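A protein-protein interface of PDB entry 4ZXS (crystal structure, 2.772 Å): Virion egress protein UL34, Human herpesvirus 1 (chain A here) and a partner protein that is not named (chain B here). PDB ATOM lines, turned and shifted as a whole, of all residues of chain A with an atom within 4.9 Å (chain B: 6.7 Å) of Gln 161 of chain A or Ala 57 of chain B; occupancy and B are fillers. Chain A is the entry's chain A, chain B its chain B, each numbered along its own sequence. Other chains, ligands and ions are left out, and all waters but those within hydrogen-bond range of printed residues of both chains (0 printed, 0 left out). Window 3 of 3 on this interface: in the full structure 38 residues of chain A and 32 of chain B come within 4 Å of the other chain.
Printed residues of chain A that touch a printed residue of chain B: Ile 117, Phe 154, Arg 156, Gln 161 and Leu 162. Of the 11 printed residues of chain B, 6 touch a printed residue of chain A.
Of the printed residues of chain B, Phe 154 of chain A touches Val 56 (3.996 Å), Ala 57 (3.9 Å) and Asp 58 (3.6 Å). Printed residues of chain B within 4 Å of Arg 156 of chain A: Ala 57 and Asp 186. Of chain B, only Val 56 and Ala 57 come within 4 Å of Gln 161 of chain A. Of the printed residues of chain A, Thr 55 of chain B touches Ile 117. Printed residues of chain A within 4 Å of Ala 57 of chain B: Phe 154 (3.9 Å), Arg 156 (3.6 Å) and Gln 161 (2.6 Å). The nearest printed residue of chain A that does not touch Thr 55 of chain B is Gln 161 of chain A (4.3 Å).
Ile 117 of chain A touches Asp 53 of chain B. CD1 of Ile 117 of chain A touches O of Thr 55 of chain B, at 3.4 Å. Phe 154 of chain A touches Val 56 of chain B (CE2 to CG2, 3.996 Å). Phe 154 of chain A touches Ala 57 of chain B (CG to CB, 3.9 Å). Asp 58 of chain B touches Phe 154 of chain A. CB of Ala 57 of chain B touches NH2 of Arg 156 of chain A, at 3.6 Å. OE1 of Gln 161 of chain A touches C of Val 56 of chain B, at 3.4 Å. Leu 162 of chain A touches Val 56 of chain B.
The backbone NH (N) of Val 56 of chain B lies close to the side-chain amide oxygen (OD1) of Asn 59 of chain B, at 3.4 Å. The backbone carbonyl oxygen of Phe 154 of chain A sits at hydrogen-bond distance from the backbone NH of Gln 161 of chain A, 2.9 Å away. The backbone NH (N) of Val 116 of chain A lies within hydrogen-bond range of the backbone carbonyl oxygen (O) of Leu 162 of chain A.
The side-chain carboxylate (OD1) of Asp 186 of chain B lies within salt-bridge range of the guanidinium group (NH1) of Arg 156 of chain A (3.3 Å). N of Ala 57 of chain B lies within hydrogen-bond range of OE1 of Gln 161 of chain A (2.6 Å).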
ATOM      1  N   VAL A 116     -13.295  22.702  22.940  1.00  0.00           N
ATOM      2  CA  VAL A 116     -13.790  23.727  22.027  1.00  0.00           C
ATOM      3  C   VAL A 116     -13.233  23.468  20.627  1.00  0.00           C
ATOM      4  O   VAL A 116     -12.016  23.439  20.431  1.00  0.00           O
ATOM      5  CB  VAL A 116     -13.403  25.155  22.475  1.00  0.00           C
ATOM      6  CG1 VAL A 116     -13.900  26.178  21.465  1.00  0.00           C
ATOM      7  CG2 VAL A 116     -13.948  25.460  23.864  1.00  0.00           C
ATOM      8  N   ILE A 117     -14.101  23.259  19.645  1.00  0.00           N
ATOM      9  CA  ILE A 117     -13.682  23.004  18.271  1.00  0.00           C
ATOM     10  C   ILE A 117     -13.974  24.198  17.411  1.00  0.00           C
ATOM     11  O   ILE A 117     -15.066  24.665  17.382  1.00  0.00           O
ATOM     12  CB  ILE A 117     -14.409  21.826  17.667  1.00  0.00           C
ATOM     13  CG1 ILE A 117     -14.399  20.649  18.611  1.00  0.00           C
ATOM     14  CG2 ILE A 117     -13.754  21.442  16.375  1.00  0.00           C
ATOM     15  CD1 ILE A 117     -13.061  20.014  18.774  1.00  0.00           C
ATOM     16  N   SER A 152      -4.555  21.767  24.917  1.00  0.00           N
ATOM     17  CA  SER A 152      -4.162  20.731  23.976  1.00  0.00           C
ATOM     18  C   SER A 152      -4.724  21.074  22.605  1.00  0.00           C
ATOM     19  O   SER A 152      -5.938  21.089  22.409  1.00  0.00           O
ATOM     20  CB  SER A 152      -4.660  19.359  24.438  1.00  0.00           C
ATOM     21  OG  SER A 152      -3.802  18.806  25.420  1.00  0.00           O
ATOM     22  N   CYS A 153      -3.836  21.349  21.655  1.00  0.00           N
ATOM     23  CA  CYS A 153      -4.258  21.802  20.337  1.00  0.00           C
ATOM     24  C   CYS A 153      -3.915  20.796  19.249  1.00  0.00           C
ATOM     25  O   CYS A 153      -2.748  20.471  19.028  1.00  0.00           O
ATOM     26  CB  CYS A 153      -3.624  23.156  20.010  1.00  0.00           C
ATOM     27  SG  CYS A 153      -4.253  23.933  18.507  1.00  0.00           S
ATOM     28  N   PHE A 154      -4.949  20.315  18.567  1.00  0.00           N
ATOM     29  CA  PHE A 154      -4.768  19.470  17.395  1.00  0.00           C
ATOM     30  C   PHE A 154      -5.248  20.212  16.156  1.00  0.00           C
ATOM     31  O   PHE A 154      -6.445  20.433  15.985  1.00  0.00           O
ATOM     32  CB  PHE A 154      -5.530  18.152  17.540  1.00  0.00           C
ATOM     33  CG  PHE A 154      -5.239  17.414  18.816  1.00  0.00           C
ATOM     34  CD1 PHE A 154      -4.137  16.580  18.911  1.00  0.00           C
ATOM     35  CD2 PHE A 154      -6.080  17.533  19.910  1.00  0.00           C
ATOM     36  CE1 PHE A 154      -3.870  15.892  20.079  1.00  0.00           C
ATOM     37  CE2 PHE A 154      -5.818  16.847  21.080  1.00  0.00           C
ATOM     38  CZ  PHE A 154      -4.712  16.026  21.165  1.00  0.00           C
ATOM     39  N   ARG A 156      -6.226  20.335  12.524  1.00  0.00           N
ATOM     40  CA  ARG A 156      -6.705  19.471  11.457  1.00  0.00           C
ATOM     41  C   ARG A 156      -7.603  20.259  10.513  1.00  0.00           C
ATOM     42  O   ARG A 156      -8.812  20.164  10.573  1.00  0.00           O
ATOM     43  CB  ARG A 156      -7.511  18.333  12.059  1.00  0.00           C
ATOM     44  CG  ARG A 156      -6.882  17.635  13.233  1.00  0.00           C
ATOM     45  CD  ARG A 156      -5.870  16.640  12.764  1.00  0.00           C
ATOM     46  NE  ARG A 156      -5.113  16.029  13.830  1.00  0.00           N
ATOM     47  CZ  ARG A 156      -5.265  14.784  14.241  1.00  0.00           C
ATOM     48  NH1 ARG A 156      -6.179  14.006  13.692  1.00  0.00           N
ATOM     49  NH2 ARG A 156      -4.498  14.321  15.204  1.00  0.00           N
ATOM     50  N   ARG A 159     -10.556  22.389  10.455  1.00  0.00           N
ATOM     51  CA  ARG A 159     -10.879  22.598  11.867  1.00  0.00           C
ATOM     52  C   ARG A 159      -9.673  22.611  12.814  1.00  0.00           C
ATOM     53  O   ARG A 159      -8.583  22.147  12.476  1.00  0.00           O
ATOM     54  CB  ARG A 159     -11.875  21.531  12.336  1.00  0.00           C
ATOM     55  CG  ARG A 159     -13.305  21.770  11.881  1.00  0.00           C
ATOM     56  CD  ARG A 159     -14.097  20.476  11.781  1.00  0.00           C
ATOM     57  NE  ARG A 159     -13.758  19.721  10.579  1.00  0.00           N
ATOM     58  CZ  ARG A 159     -14.431  19.800   9.435  1.00  0.00           C
ATOM     59  NH1 ARG A 159     -15.489  20.596   9.339  1.00  0.00           N
ATOM     60  NH2 ARG A 159     -14.053  19.078   8.390  1.00  0.00           N
ATOM     61  N   VAL A 160      -9.890  23.156  14.008  1.00  0.00           N
ATOM     62  CA  VAL A 160      -8.892  23.136  15.074  1.00  0.00           C
ATOM     63  C   VAL A 160      -9.509  22.632  16.377  1.00  0.00           C
ATOM     64  O   VAL A 160     -10.510  23.177  16.847  1.00  0.00           O
ATOM     65  CB  VAL A 160      -8.274  24.531  15.303  1.00  0.00           C
ATOM     66  CG1 VAL A 160      -7.417  24.535  16.558  1.00  0.00           C
ATOM     67  CG2 VAL A 160      -7.457  24.961  14.096  1.00  0.00           C
ATOM     68  N   GLN A 161      -8.908  21.601  16.964  1.00  0.00           N
ATOM     69  CA  GLN A 161      -9.427  21.028  18.204  1.00  0.00           C
ATOM     70  C   GLN A 161      -8.679  21.548  19.429  1.00  0.00           C
ATOM     71  O   GLN A 161      -7.452  21.466  19.503  1.00  0.00           O
ATOM     72  CB  GLN A 161      -9.353  19.500  18.164  1.00  0.00           C
ATOM     73  CG  GLN A 161      -9.696  18.893  16.815  1.00  0.00           C
ATOM     74  CD  GLN A 161      -9.470  17.396  16.783  1.00  0.00           C
ATOM     75  OE1 GLN A 161      -8.650  16.864  17.532  1.00  0.00           O
ATOM     76  NE2 GLN A 161     -10.198  16.705  15.913  1.00  0.00           N
ATOM     77  N   LEU A 162      -9.430  22.092  20.383  1.00  0.00           N
ATOM     78  CA  LEU A 162      -8.851  22.620  21.615  1.00  0.00           C
ATOM     79  C   LEU A 162      -9.382  21.891  22.846  1.00  0.00           C
ATOM     80  O   LEU A 162     -10.586  21.694  22.990  1.00  0.00           O
ATOM     81  CB  LEU A 162      -9.129  24.118  21.740  1.00  0.00           C
ATOM     82  CG  LEU A 162      -8.665  24.999  20.581  1.00  0.00           C
ATOM     83  CD1 LEU A 162      -9.172  26.413  20.769  1.00  0.00           C
ATOM     84  CD2 LEU A 162      -7.152  24.983  20.468  1.00  0.00           C
ATOM     85  N   ALA A 163      -8.473  21.487  23.729  1.00  0.00           N
ATOM     86  CA  ALA A 163      -8.849  20.850  24.985  1.00  0.00           C
ATOM     87  C   ALA A 163      -8.211  21.566  26.171  1.00  0.00           C
ATOM     88  O   ALA A 163      -7.016  21.416  26.429  1.00  0.00           O
ATOM     89  CB  ALA A 163      -8.453  19.384  24.974  1.00  0.00           C
ATOM     90  N   ASP B  53     -17.986  15.027  16.654  1.00  0.00           N
ATOM     91  CA  ASP B  53     -17.201  16.131  16.163  1.00  0.00           C
ATOM     92  C   ASP B  53     -16.759  16.973  17.323  1.00  0.00           C
ATOM     93  O   ASP B  53     -15.853  17.743  17.199  1.00  0.00           O
ATOM     94  CB  ASP B  53     -17.957  16.962  15.134  1.00  0.00           C
ATOM     95  CG  ASP B  53     -19.283  17.386  15.599  1.00  0.00           C
ATOM     96  OD1 ASP B  53     -19.694  16.989  16.672  1.00  0.00           O
ATOM     97  OD2 ASP B  53     -19.932  18.132  14.888  1.00  0.00           O
ATOM     98  N   THR B  55     -15.349  15.973  19.963  1.00  0.00           N
ATOM     99  CA  THR B  55     -14.273  15.307  20.608  1.00  0.00           C
ATOM    100  C   THR B  55     -13.001  15.893  20.080  1.00  0.00           C
ATOM    101  O   THR B  55     -13.005  16.619  19.143  1.00  0.00           O
ATOM    102  CB  THR B  55     -14.273  13.815  20.245  1.00  0.00           C
ATOM    103  OG1 THR B  55     -14.472  13.657  18.854  1.00  0.00           O
ATOM    104  CG2 THR B  55     -15.372  13.143  20.890  1.00  0.00           C
ATOM    105  N   VAL B  56     -11.906  15.557  20.703  1.00  0.00           N
ATOM    106  CA  VAL B  56     -10.588  15.978  20.269  1.00  0.00           C
ATOM    107  C   VAL B  56      -9.821  14.729  19.934  1.00  0.00           C
ATOM    108  O   VAL B  56     -10.127  13.707  20.438  1.00  0.00           O
ATOM    109  CB  VAL B  56      -9.826  16.819  21.296  1.00  0.00           C
ATOM    110  CG1 VAL B  56     -10.583  18.082  21.599  1.00  0.00           C
ATOM    111  CG2 VAL B  56      -9.452  16.027  22.526  1.00  0.00           C
ATOM    112  N   ALA B  57      -8.828  14.813  19.080  1.00  0.00           N
ATOM    113  CA  ALA B  57      -8.091  13.644  18.628  1.00  0.00           C
ATOM    114  C   ALA B  57      -7.680  12.539  19.589  1.00  0.00           C
ATOM    115  O   ALA B  57      -7.491  11.430  19.175  1.00  0.00           O
ATOM    116  CB  ALA B  57      -6.920  14.065  17.788  1.00  0.00           C
ATOM    117  N   ASP B  58      -7.517  12.843  20.857  1.00  0.00           N
ATOM    118  CA  ASP B  58      -7.125  11.865  21.870  1.00  0.00           C
ATOM    119  C   ASP B  58      -8.254  11.533  22.849  1.00  0.00           C
ATOM    120  O   ASP B  58      -8.009  10.975  23.920  1.00  0.00           O
ATOM    121  CB  ASP B  58      -5.891  12.352  22.641  1.00  0.00           C
ATOM    122  CG  ASP B  58      -6.189  13.537  23.538  1.00  0.00           C
ATOM    123  OD1 ASP B  58      -7.150  14.276  23.248  1.00  0.00           O
ATOM    124  OD2 ASP B  58      -5.466  13.725  24.539  1.00  0.00           O
ATOM    125  N   ASN B  59      -9.476  11.811  22.485  1.00  0.00           N
ATOM    126  CA  ASN B  59     -10.583  11.488  23.341  1.00  0.00           C
ATOM    127  C   ASN B  59     -11.235  10.172  23.086  1.00  0.00           C
ATOM    128  O   ASN B  59     -11.476   9.804  21.977  1.00  0.00           O
ATOM    129  CB  ASN B  59     -11.655  12.496  23.164  1.00  0.00           C
ATOM    130  CG  ASN B  59     -11.620  13.544  24.180  1.00  0.00           C
ATOM    131  OD1 ASN B  59     -12.036  14.617  23.921  1.00  0.00           O
ATOM    132  ND2 ASN B  59     -11.151  13.237  25.345  1.00  0.00           N
ATOM    133  N   TYR B 182      -9.823   6.140  21.338  1.00  0.00           N
ATOM    134  CA  TYR B 182      -9.575   7.424  20.742  1.00  0.00           C
ATOM    135  C   TYR B 182      -9.105   7.321  19.325  1.00  0.00           C
ATOM    136  O   TYR B 182      -9.493   8.064  18.473  1.00  0.00           O
ATOM    137  CB  TYR B 182      -8.621   8.236  21.612  1.00  0.00           C
ATOM    138  CG  TYR B 182      -7.192   7.799  21.644  1.00  0.00           C
ATOM    139  CD1 TYR B 182      -6.783   6.786  22.449  1.00  0.00           C
ATOM    140  CD2 TYR B 182      -6.251   8.437  20.905  1.00  0.00           C
ATOM    141  CE1 TYR B 182      -5.473   6.397  22.495  1.00  0.00           C
ATOM    142  CE2 TYR B 182      -4.951   8.048  20.933  1.00  0.00           C
ATOM    143  CZ  TYR B 182      -4.574   7.033  21.736  1.00  0.00           C
ATOM    144  OH  TYR B 182      -3.281   6.655  21.758  1.00  0.00           O
ATOM    145  N   ARG B 183      -8.247   6.370  19.085  1.00  0.00           N
ATOM    146  CA  ARG B 183      -7.710   6.104  17.761  1.00  0.00           C
ATOM    147  C   ARG B 183      -8.833   5.732  16.797  1.00  0.00           C
ATOM    148  O   ARG B 183      -8.831   6.138  15.632  1.00  0.00           O
ATOM    149  CB  ARG B 183      -6.675   4.979  17.835  1.00  0.00           C
ATOM    150  CG  ARG B 183      -5.333   5.419  18.394  1.00  0.00           C
ATOM    151  CD  ARG B 183      -4.208   4.484  17.987  1.00  0.00           C
ATOM    152  NE  ARG B 183      -2.905   5.140  18.065  1.00  0.00           N
ATOM    153  CZ  ARG B 183      -2.174   5.224  19.171  1.00  0.00           C
ATOM    154  NH1 ARG B 183      -2.622   4.700  20.304  1.00  0.00           N
ATOM    155  NH2 ARG B 183      -1.000   5.840  19.147  1.00  0.00           N
ATOM    156  N   ILE B 185     -12.076   6.623  17.060  1.00  0.00           N
ATOM    157  CA  ILE B 185     -12.918   7.786  16.812  1.00  0.00           C
ATOM    158  C   ILE B 185     -12.233   8.730  15.831  1.00  0.00           C
ATOM    159  O   ILE B 185     -12.859   9.242  14.898  1.00  0.00           O
ATOM    160  CB  ILE B 185     -13.236   8.540  18.117  1.00  0.00           C
ATOM    161  CG1 ILE B 185     -13.975   7.625  19.095  1.00  0.00           C
ATOM    162  CG2 ILE B 185     -14.049   9.795  17.828  1.00  0.00           C
ATOM    163  CD1 ILE B 185     -14.422   8.316  20.362  1.00  0.00           C
ATOM    164  N   ASP B 186     -10.937   8.937  16.043  1.00  0.00           N
ATOM    165  CA  ASP B 186     -10.143   9.795  15.176  1.00  0.00           C
ATOM    166  C   ASP B 186     -10.158   9.254  13.751  1.00  0.00           C
ATOM    167  O   ASP B 186     -10.431   9.989  12.796  1.00  0.00           O
ATOM    168  CB  ASP B 186      -8.707   9.901  15.693  1.00  0.00           C
ATOM    169  CG  ASP B 186      -7.956  11.080  15.103  1.00  0.00           C
ATOM    170  OD1 ASP B 186      -8.590  12.127  14.850  1.00  0.00           O
ATOM    171  OD2 ASP B 186      -6.730  10.959  14.894  1.00  0.00           O
ATOM    172  N   LEU B 189     -13.656   9.538  12.094  1.00  0.00           N
ATOM    173  CA  LEU B 189     -13.963  10.905  11.682  1.00  0.00           C
ATOM    174  C   LEU B 189     -13.156  11.323  10.455  1.00  0.00           C
ATOM    175  O   LEU B 189     -13.695  11.926   9.527  1.00  0.00           O
ATOM    176  CB  LEU B 189     -13.709  11.884  12.831  1.00  0.00           C
ATOM    177  CG  LEU B 189     -14.645  11.797  14.039  1.00  0.00           C
ATOM    178  CD1 LEU B 189     -14.233  12.795  15.107  1.00  0.00           C
ATOM    179  CD2 LEU B 189     -16.082  12.032  13.614  1.00  0.00           C
